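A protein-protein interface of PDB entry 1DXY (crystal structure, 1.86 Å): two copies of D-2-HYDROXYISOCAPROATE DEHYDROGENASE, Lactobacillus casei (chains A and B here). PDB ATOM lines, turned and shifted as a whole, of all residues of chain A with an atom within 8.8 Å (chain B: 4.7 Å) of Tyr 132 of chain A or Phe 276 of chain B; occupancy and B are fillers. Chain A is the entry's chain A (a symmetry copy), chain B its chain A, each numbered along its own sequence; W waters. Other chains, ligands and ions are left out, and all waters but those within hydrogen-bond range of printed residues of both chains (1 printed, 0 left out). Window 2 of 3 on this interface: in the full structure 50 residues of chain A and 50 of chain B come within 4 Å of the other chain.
Of the 13 printed residues of chain B, 6 touch a printed residue of chain A.
Of the 15 printed residues of chain A, 5 touch a printed residue of chain B.
Hydrophobic or aromatic side chains of chain A that line the printed part of chain B: Val 123, Tyr 132 and Ala 135.
Among the printed residues, no Asp or Glu carboxylate lies within 4 Å of a Lys or Arg side-chain nitrogen of the other chain.
The side-chain carboxylate (OE2) of Glu 263 of chain B is in hydrogen-bond range of the side-chain hydroxyl (OH) of Tyr 132 of chain A.
Water W1 lies within hydrogen-bond range of O of Leu 127 of chain A (3.0 Å) and NE1 of Trp 281 of chain B (3.1 Å).
No position is printed for both chains.
Of the 9 pairs that touch across the chains among the printed residues, none has its exchanged pair printed and touching as well.
OD1 of Asp 278 of chain B sits at hydrogen-bond distance from N of Trp 281 of chain B, at 3.2 Å.
The side-chain carboxylate of Asp 131 of chain A lies close to the backbone NH of Glu 133 of chain A (3.4 Å).
O of Phe 276 of chain B sits at hydrogen-bond distance from ND2 of Asn 269 of chain B (2.9 Å).
ND1 of His 295 of chain B lies within hydrogen-bond range of OE1 of Glu 263 of chain B (3.1 Å).
N of Leu 270 of chain B is in hydrogen-bond range of O of Ser 275 of chain B.
Among the printed residues, merely in contact across the chains: Val 123 of chain A with Pro 294 of chain B, Tyr 132 of chain A with Leu 267 of chain B, Tyr 132 of chain A with Phe 276 of chain B, Tyr 132 of chain A with Trp 281 of chain B, Tyr 132 of chain A with Pro 294 of chain B, Glu 133 of chain A with Leu 270 of chain B, Ala 135 of chain A with Pro 294 of chain B and Gly 136 of chain A with Pro 294 of chain B.
Ala 129 of chain A touches none of the printed residues of chain B.
Of chain B, only Glu 263, Leu 267, Phe 276, Trp 281 and Pro 294 come within 4 Å of Tyr 132 of chain A.
Of the printed residues of chain B, Gly 136 of chain A touches Pro 294 (3.8 Å).
Printed residues of chain A within 4 Å of Leu 270 of chain B: Glu 133.
Asp 278 of chain B touches none of the printed residues of chain A.
The nearest printed residue of chain B that does not touch Gly 136 of chain A is His 295 of chain B (6.8 Å).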
ATOM      1  N   VAL A 123       7.115  -4.599 -10.520  1.00  0.00           N
ATOM      2  CA  VAL A 123       6.867  -3.530 -11.462  1.00  0.00           C
ATOM      3  C   VAL A 123       8.112  -3.244 -12.284  1.00  0.00           C
ATOM      4  O   VAL A 123       8.042  -3.180 -13.516  1.00  0.00           O
ATOM      5  CB  VAL A 123       6.411  -2.238 -10.748  1.00  0.00           C
ATOM      6  CG1 VAL A 123       6.358  -1.066 -11.740  1.00  0.00           C
ATOM      7  CG2 VAL A 123       5.055  -2.450 -10.109  1.00  0.00           C
ATOM      8  N   ALA A 125      10.720  -5.142 -12.843  1.00  0.00           N
ATOM      9  CA  ALA A 125      11.104  -6.275 -13.682  1.00  0.00           C
ATOM     10  C   ALA A 125      10.311  -6.273 -14.986  1.00  0.00           C
ATOM     11  O   ALA A 125      10.863  -6.510 -16.064  1.00  0.00           O
ATOM     12  CB  ALA A 125      10.903  -7.592 -12.939  1.00  0.00           C
ATOM     13  N   GLN A 126       9.020  -5.976 -14.897  1.00  0.00           N
ATOM     14  CA  GLN A 126       8.182  -5.949 -16.091  1.00  0.00           C
ATOM     15  C   GLN A 126       8.496  -4.777 -17.012  1.00  0.00           C
ATOM     16  O   GLN A 126       8.465  -4.928 -18.233  1.00  0.00           O
ATOM     17  CB  GLN A 126       6.699  -5.955 -15.728  1.00  0.00           C
ATOM     18  CG  GLN A 126       6.237  -7.252 -15.124  1.00  0.00           C
ATOM     19  CD  GLN A 126       6.473  -8.448 -16.038  1.00  0.00           C
ATOM     20  OE1 GLN A 126       6.357  -8.351 -17.256  1.00  0.00           O
ATOM     21  NE2 GLN A 126       6.789  -9.588 -15.447  1.00  0.00           N
ATOM     22  N   LEU A 127       8.804  -3.611 -16.450  1.00  0.00           N
ATOM     23  CA  LEU A 127       9.118  -2.468 -17.291  1.00  0.00           C
ATOM     24  C   LEU A 127      10.407  -2.738 -18.051  1.00  0.00           C
ATOM     25  O   LEU A 127      10.489  -2.469 -19.254  1.00  0.00           O
ATOM     26  CB  LEU A 127       9.251  -1.179 -16.477  1.00  0.00           C
ATOM     27  CG  LEU A 127       8.005  -0.581 -15.827  1.00  0.00           C
ATOM     28  CD1 LEU A 127       8.422   0.710 -15.169  1.00  0.00           C
ATOM     29  CD2 LEU A 127       6.908  -0.318 -16.846  1.00  0.00           C
ATOM     30  N   GLN A 128      11.396  -3.296 -17.359  1.00  0.00           N
ATOM     31  CA  GLN A 128      12.676  -3.600 -17.984  1.00  0.00           C
ATOM     32  C   GLN A 128      12.512  -4.632 -19.094  1.00  0.00           C
ATOM     33  O   GLN A 128      13.210  -4.583 -20.095  1.00  0.00           O
ATOM     34  CB  GLN A 128      13.704  -4.065 -16.948  1.00  0.00           C
ATOM     35  CG  GLN A 128      14.168  -2.967 -15.986  1.00  0.00           C
ATOM     36  CD  GLN A 128      14.816  -1.777 -16.701  1.00  0.00           C
ATOM     37  OE1 GLN A 128      15.195  -1.878 -17.871  1.00  0.00           O
ATOM     38  NE2 GLN A 128      14.962  -0.656 -15.999  1.00  0.00           N
ATOM     39  N   ALA A 129      11.555  -5.538 -18.928  1.00  0.00           N
ATOM     40  CA  ALA A 129      11.283  -6.567 -19.925  1.00  0.00           C
ATOM     41  C   ALA A 129      10.429  -5.999 -21.069  1.00  0.00           C
ATOM     42  O   ALA A 129      10.063  -6.713 -21.999  1.00  0.00           O
ATOM     43  CB  ALA A 129      10.568  -7.738 -19.269  1.00  0.00           C
ATOM     44  N   GLY A 130      10.095  -4.714 -20.978  1.00  0.00           N
ATOM     45  CA  GLY A 130       9.287  -4.081 -21.997  1.00  0.00           C
ATOM     46  C   GLY A 130       7.795  -4.363 -21.927  1.00  0.00           C
ATOM     47  O   GLY A 130       7.096  -4.134 -22.904  1.00  0.00           O
ATOM     48  N   ASP A 131       7.273  -4.838 -20.801  1.00  0.00           N
ATOM     49  CA  ASP A 131       5.840  -5.100 -20.716  1.00  0.00           C
ATOM     50  C   ASP A 131       5.135  -4.096 -19.802  1.00  0.00           C
ATOM     51  O   ASP A 131       4.825  -4.386 -18.640  1.00  0.00           O
ATOM     52  CB  ASP A 131       5.579  -6.536 -20.256  1.00  0.00           C
ATOM     53  CG  ASP A 131       4.157  -6.994 -20.544  1.00  0.00           C
ATOM     54  OD1 ASP A 131       3.259  -6.136 -20.707  1.00  0.00           O
ATOM     55  OD2 ASP A 131       3.929  -8.218 -20.600  1.00  0.00           O
ATOM     56  N   TYR A 132       4.832  -2.929 -20.359  1.00  0.00           N
ATOM     57  CA  TYR A 132       4.182  -1.859 -19.624  1.00  0.00           C
ATOM     58  C   TYR A 132       2.822  -2.243 -19.077  1.00  0.00           C
ATOM     59  O   TYR A 132       2.460  -1.824 -17.978  1.00  0.00           O
ATOM     60  CB  TYR A 132       4.067  -0.621 -20.505  1.00  0.00           C
ATOM     61  CG  TYR A 132       3.610   0.630 -19.790  1.00  0.00           C
ATOM     62  CD1 TYR A 132       2.251   0.933 -19.666  1.00  0.00           C
ATOM     63  CD2 TYR A 132       4.541   1.545 -19.292  1.00  0.00           C
ATOM     64  CE1 TYR A 132       1.829   2.123 -19.072  1.00  0.00           C
ATOM     65  CE2 TYR A 132       4.130   2.737 -18.698  1.00  0.00           C
ATOM     66  CZ  TYR A 132       2.777   3.020 -18.594  1.00  0.00           C
ATOM     67  OH  TYR A 132       2.382   4.210 -18.033  1.00  0.00           O
ATOM     68  N   GLU A 133       2.062  -3.036 -19.820  1.00  0.00           N
ATOM     69  CA  GLU A 133       0.748  -3.429 -19.343  1.00  0.00           C
ATOM     70  C   GLU A 133       0.845  -4.358 -18.146  1.00  0.00           C
ATOM     71  O   GLU A 133       0.148  -4.166 -17.146  1.00  0.00           O
ATOM     72  CB  GLU A 133      -0.071  -4.083 -20.452  1.00  0.00           C
ATOM     73  CG  GLU A 133      -0.418  -3.101 -21.557  1.00  0.00           C
ATOM     74  CD  GLU A 133      -1.372  -3.673 -22.610  1.00  0.00           C
ATOM     75  OE1 GLU A 133      -1.115  -4.801 -23.123  1.00  0.00           O
ATOM     76  OE2 GLU A 133      -2.372  -2.979 -22.927  1.00  0.00           O
ATOM     77  N   LYS A 134       1.722  -5.352 -18.226  1.00  0.00           N
ATOM     78  CA  LYS A 134       1.860  -6.278 -17.116  1.00  0.00           C
ATOM     79  C   LYS A 134       2.443  -5.590 -15.873  1.00  0.00           C
ATOM     80  O   LYS A 134       2.098  -5.955 -14.748  1.00  0.00           O
ATOM     81  CB  LYS A 134       2.687  -7.503 -17.506  1.00  0.00           C
ATOM     82  CG  LYS A 134       2.523  -8.633 -16.523  1.00  0.00           C
ATOM     83  CD  LYS A 134       2.806  -9.966 -17.152  1.00  0.00           C
ATOM     84  CE  LYS A 134       2.461 -11.094 -16.186  1.00  0.00           C
ATOM     85  NZ  LYS A 134       2.369 -12.430 -16.876  1.00  0.00           N
ATOM     86  N   ALA A 135       3.269  -4.566 -16.077  1.00  0.00           N
ATOM     87  CA  ALA A 135       3.875  -3.831 -14.974  1.00  0.00           C
ATOM     88  C   ALA A 135       2.823  -3.183 -14.077  1.00  0.00           C
ATOM     89  O   ALA A 135       3.100  -2.864 -12.915  1.00  0.00           O
ATOM     90  CB  ALA A 135       4.821  -2.776 -15.499  1.00  0.00           C
ATOM     91  N   GLY A 136       1.613  -2.996 -14.607  1.00  0.00           N
ATOM     92  CA  GLY A 136       0.554  -2.378 -13.830  1.00  0.00           C
ATOM     93  C   GLY A 136      -0.506  -3.345 -13.345  1.00  0.00           C
ATOM     94  O   GLY A 136      -1.641  -2.950 -13.095  1.00  0.00           O
ATOM     95  N   THR A 137      -0.139  -4.607 -13.156  1.00  0.00           N
ATOM     96  CA  THR A 137      -1.117  -5.583 -12.721  1.00  0.00           C
ATOM     97  C   THR A 137      -0.886  -6.151 -11.329  1.00  0.00           C
ATOM     98  O   THR A 137      -1.556  -7.109 -10.945  1.00  0.00           O
ATOM     99  CB  THR A 137      -1.193  -6.749 -13.718  1.00  0.00           C
ATOM    100  OG1 THR A 137       0.075  -7.406 -13.763  1.00  0.00           O
ATOM    101  CG2 THR A 137      -1.533  -6.235 -15.125  1.00  0.00           C
ATOM    102  N   PHE A 138       0.031  -5.563 -10.564  1.00  0.00           N
ATOM    103  CA  PHE A 138       0.324  -6.054  -9.214  1.00  0.00           C
ATOM    104  C   PHE A 138      -0.239  -5.107  -8.167  1.00  0.00           C
ATOM    105  O   PHE A 138       0.497  -4.283  -7.617  1.00  0.00           O
ATOM    106  CB  PHE A 138       1.835  -6.171  -9.038  1.00  0.00           C
ATOM    107  CG  PHE A 138       2.499  -6.922 -10.136  1.00  0.00           C
ATOM    108  CD1 PHE A 138       2.318  -8.293 -10.260  1.00  0.00           C
ATOM    109  CD2 PHE A 138       3.283  -6.258 -11.067  1.00  0.00           C
ATOM    110  CE1 PHE A 138       2.912  -8.997 -11.306  1.00  0.00           C
ATOM    111  CE2 PHE A 138       3.881  -6.951 -12.117  1.00  0.00           C
ATOM    112  CZ  PHE A 138       3.694  -8.323 -12.236  1.00  0.00           C
ATOM    113  N   GLU B 263       2.753   9.228 -22.038  1.00  0.00           N
ATOM    114  CA  GLU B 263       2.109   7.948 -21.804  1.00  0.00           C
ATOM    115  C   GLU B 263       1.017   7.612 -22.831  1.00  0.00           C
ATOM    116  O   GLU B 263       1.006   6.509 -23.396  1.00  0.00           O
ATOM    117  CB  GLU B 263       1.515   7.909 -20.397  1.00  0.00           C
ATOM    118  CG  GLU B 263       0.686   6.668 -20.136  1.00  0.00           C
ATOM    119  CD  GLU B 263       0.005   6.676 -18.786  1.00  0.00           C
ATOM    120  OE1 GLU B 263      -0.210   7.773 -18.201  1.00  0.00           O
ATOM    121  OE2 GLU B 263      -0.310   5.565 -18.311  1.00  0.00           O
ATOM    122  N   ASP B 266       2.386   6.939 -26.296  1.00  0.00           N
ATOM    123  CA  ASP B 266       3.107   5.667 -26.231  1.00  0.00           C
ATOM    124  C   ASP B 266       2.213   4.433 -26.129  1.00  0.00           C
ATOM    125  O   ASP B 266       2.562   3.382 -26.672  1.00  0.00           O
ATOM    126  CB  ASP B 266       4.133   5.668 -25.090  1.00  0.00           C
ATOM    127  CG  ASP B 266       5.356   6.538 -25.383  1.00  0.00           C
ATOM    128  OD1 ASP B 266       5.361   7.300 -26.377  1.00  0.00           O
ATOM    129  OD2 ASP B 266       6.325   6.460 -24.595  1.00  0.00           O
ATOM    130  N   LEU B 267       1.086   4.535 -25.423  1.00  0.00           N
ATOM    131  CA  LEU B 267       0.176   3.395 -25.302  1.00  0.00           C
ATOM    132  C   LEU B 267      -0.462   3.097 -26.670  1.00  0.00           C
ATOM    133  O   LEU B 267      -0.801   1.948 -26.991  1.00  0.00           O
ATOM    134  CB  LEU B 267      -0.901   3.659 -24.246  1.00  0.00           C
ATOM    135  CG  LEU B 267      -0.478   3.536 -22.775  1.00  0.00           C
ATOM    136  CD1 LEU B 267      -1.601   4.006 -21.872  1.00  0.00           C
ATOM    137  CD2 LEU B 267      -0.101   2.089 -22.456  1.00  0.00           C
ATOM    138  N   ASN B 269       1.127   3.692 -29.603  1.00  0.00           N
ATOM    139  CA  ASN B 269       2.205   3.038 -30.353  1.00  0.00           C
ATOM    140  C   ASN B 269       2.322   1.588 -29.930  1.00  0.00           C
ATOM    141  O   ASN B 269       2.542   0.715 -30.763  1.00  0.00           O
ATOM    142  CB  ASN B 269       3.563   3.700 -30.107  1.00  0.00           C
ATOM    143  CG  ASN B 269       3.686   5.057 -30.759  1.00  0.00           C
ATOM    144  OD1 ASN B 269       2.902   5.416 -31.649  1.00  0.00           O
ATOM    145  ND2 ASN B 269       4.690   5.818 -30.339  1.00  0.00           N
ATOM    146  N   LEU B 270       2.236   1.339 -28.628  1.00  0.00           N
ATOM    147  CA  LEU B 270       2.315  -0.017 -28.109  1.00  0.00           C
ATOM    148  C   LEU B 270       1.240  -0.902 -28.771  1.00  0.00           C
ATOM    149  O   LEU B 270       1.528  -2.020 -29.194  1.00  0.00           O
ATOM    150  CB  LEU B 270       2.147  -0.017 -26.579  1.00  0.00           C
ATOM    151  CG  LEU B 270       2.113  -1.389 -25.892  1.00  0.00           C
ATOM    152  CD1 LEU B 270       3.501  -2.018 -25.976  1.00  0.00           C
ATOM    153  CD2 LEU B 270       1.639  -1.263 -24.442  1.00  0.00           C
ATOM    154  N   SER B 275       5.390  -1.658 -29.265  1.00  0.00           N
ATOM    155  CA  SER B 275       6.513  -0.999 -28.608  1.00  0.00           C
ATOM    156  C   SER B 275       6.174   0.482 -28.436  1.00  0.00           C
ATOM    157  O   SER B 275       5.368   1.034 -29.181  1.00  0.00           O
ATOM    158  CB  SER B 275       7.767  -1.141 -29.480  1.00  0.00           C
ATOM    159  OG  SER B 275       8.754  -0.182 -29.139  1.00  0.00           O
ATOM    160  N   PHE B 276       6.797   1.127 -27.464  1.00  0.00           N
ATOM    161  CA  PHE B 276       6.556   2.541 -27.237  1.00  0.00           C
ATOM    162  C   PHE B 276       7.125   3.409 -28.350  1.00  0.00           C
ATOM    163  O   PHE B 276       6.595   4.489 -28.611  1.00  0.00           O
ATOM    164  CB  PHE B 276       7.169   2.989 -25.908  1.00  0.00           C
ATOM    165  CG  PHE B 276       6.260   2.820 -24.721  1.00  0.00           C
ATOM    166  CD1 PHE B 276       5.066   2.103 -24.824  1.00  0.00           C
ATOM    167  CD2 PHE B 276       6.583   3.411 -23.498  1.00  0.00           C
ATOM    168  CE1 PHE B 276       4.208   1.981 -23.731  1.00  0.00           C
ATOM    169  CE2 PHE B 276       5.733   3.294 -22.400  1.00  0.00           C
ATOM    170  CZ  PHE B 276       4.544   2.579 -22.520  1.00  0.00           C
ATOM    171  N   LYS B 277       8.204   2.946 -28.994  1.00  0.00           N
ATOM    172  CA  LYS B 277       8.876   3.708 -30.062  1.00  0.00           C
ATOM    173  C   LYS B 277       9.225   5.086 -29.495  1.00  0.00           C
ATOM    174  O   LYS B 277       9.129   6.107 -30.185  1.00  0.00           O
ATOM    175  CB  LYS B 277       7.963   3.884 -31.296  1.00  0.00           C
ATOM    176  CG  LYS B 277       7.591   2.596 -32.019  1.00  0.00           C
ATOM    177  CD  LYS B 277       8.832   1.905 -32.576  1.00  0.00           C
ATOM    178  CE  LYS B 277       8.490   0.598 -33.311  1.00  0.00           C
ATOM    179  NZ  LYS B 277       9.706  -0.133 -33.819  1.00  0.00           N
ATOM    180  N   ASP B 278       9.614   5.103 -28.223  1.00  0.00           N
ATOM    181  CA  ASP B 278       9.936   6.340 -27.524  1.00  0.00           C
ATOM    182  C   ASP B 278      11.345   6.274 -26.949  1.00  0.00           C
ATOM    183  O   ASP B 278      11.569   5.648 -25.908  1.00  0.00           O
ATOM    184  CB  ASP B 278       8.911   6.560 -26.408  1.00  0.00           C
ATOM    185  CG  ASP B 278       8.995   7.939 -25.782  1.00  0.00           C
ATOM    186  OD1 ASP B 278      10.022   8.636 -25.933  1.00  0.00           O
ATOM    187  OD2 ASP B 278       8.013   8.327 -25.126  1.00  0.00           O
ATOM    188  N   TRP B 281      11.725   7.683 -23.361  1.00  0.00           N
ATOM    189  CA  TRP B 281      11.303   6.692 -22.400  1.00  0.00           C
ATOM    190  C   TRP B 281      12.467   5.723 -22.165  1.00  0.00           C
ATOM    191  O   TRP B 281      12.879   5.507 -21.027  1.00  0.00           O
ATOM    192  CB  TRP B 281      10.083   5.938 -22.932  1.00  0.00           C
ATOM    193  CG  TRP B 281       9.761   4.704 -22.147  1.00  0.00           C
ATOM    194  CD1 TRP B 281      10.166   3.422 -22.415  1.00  0.00           C
ATOM    195  CD2 TRP B 281       9.022   4.641 -20.923  1.00  0.00           C
ATOM    196  NE1 TRP B 281       9.733   2.573 -21.425  1.00  0.00           N
ATOM    197  CE2 TRP B 281       9.032   3.293 -20.497  1.00  0.00           C
ATOM    198  CE3 TRP B 281       8.360   5.595 -20.139  1.00  0.00           C
ATOM    199  CZ2 TRP B 281       8.406   2.877 -19.327  1.00  0.00           C
ATOM    200  CZ3 TRP B 281       7.734   5.176 -18.969  1.00  0.00           C
ATOM    201  CH2 TRP B 281       7.764   3.830 -18.576  1.00  0.00           C
ATOM    202  N   SER B 293       6.978   4.322 -13.152  1.00  0.00           N
ATOM    203  CA  SER B 293       5.936   3.376 -12.788  1.00  0.00           C
ATOM    204  C   SER B 293       4.806   3.640 -13.786  1.00  0.00           C
ATOM    205  O   SER B 293       4.591   4.780 -14.207  1.00  0.00           O
ATOM    206  CB  SER B 293       5.492   3.556 -11.335  1.00  0.00           C
ATOM    207  OG  SER B 293       5.309   4.914 -11.020  1.00  0.00           O
ATOM    208  N   PRO B 294       4.071   2.592 -14.167  1.00  0.00           N
ATOM    209  CA  PRO B 294       2.979   2.734 -15.139  1.00  0.00           C
ATOM    210  C   PRO B 294       1.664   3.278 -14.599  1.00  0.00           C
ATOM    211  O   PRO B 294       0.648   2.585 -14.616  1.00  0.00           O
ATOM    212  CB  PRO B 294       2.832   1.314 -15.672  1.00  0.00           C
ATOM    213  CG  PRO B 294       3.044   0.486 -14.417  1.00  0.00           C
ATOM    214  CD  PRO B 294       4.221   1.188 -13.728  1.00  0.00           C
ATOM    215  N   HIS B 295       1.694   4.495 -14.078  1.00  0.00           N
ATOM    216  CA  HIS B 295       0.487   5.131 -13.563  1.00  0.00           C
ATOM    217  C   HIS B 295      -0.237   4.258 -12.542  1.00  0.00           C
ATOM    218  O   HIS B 295      -1.436   3.978 -12.690  1.00  0.00           O
ATOM    219  CB  HIS B 295      -0.457   5.453 -14.740  1.00  0.00           C
ATOM    220  CG  HIS B 295      -1.382   6.602 -14.482  1.00  0.00           C
ATOM    221  ND1 HIS B 295      -1.588   7.612 -15.398  1.00  0.00           N
ATOM    222  CD2 HIS B 295      -2.147   6.910 -13.409  1.00  0.00           C
ATOM    223  CE1 HIS B 295      -2.437   8.493 -14.899  1.00  0.00           C
ATOM    224  NE2 HIS B 295      -2.793   8.090 -13.692  1.00  0.00           N
HETATM  225  O   HOH W   1       9.627  -0.494 -21.274  1.00  0.00           O
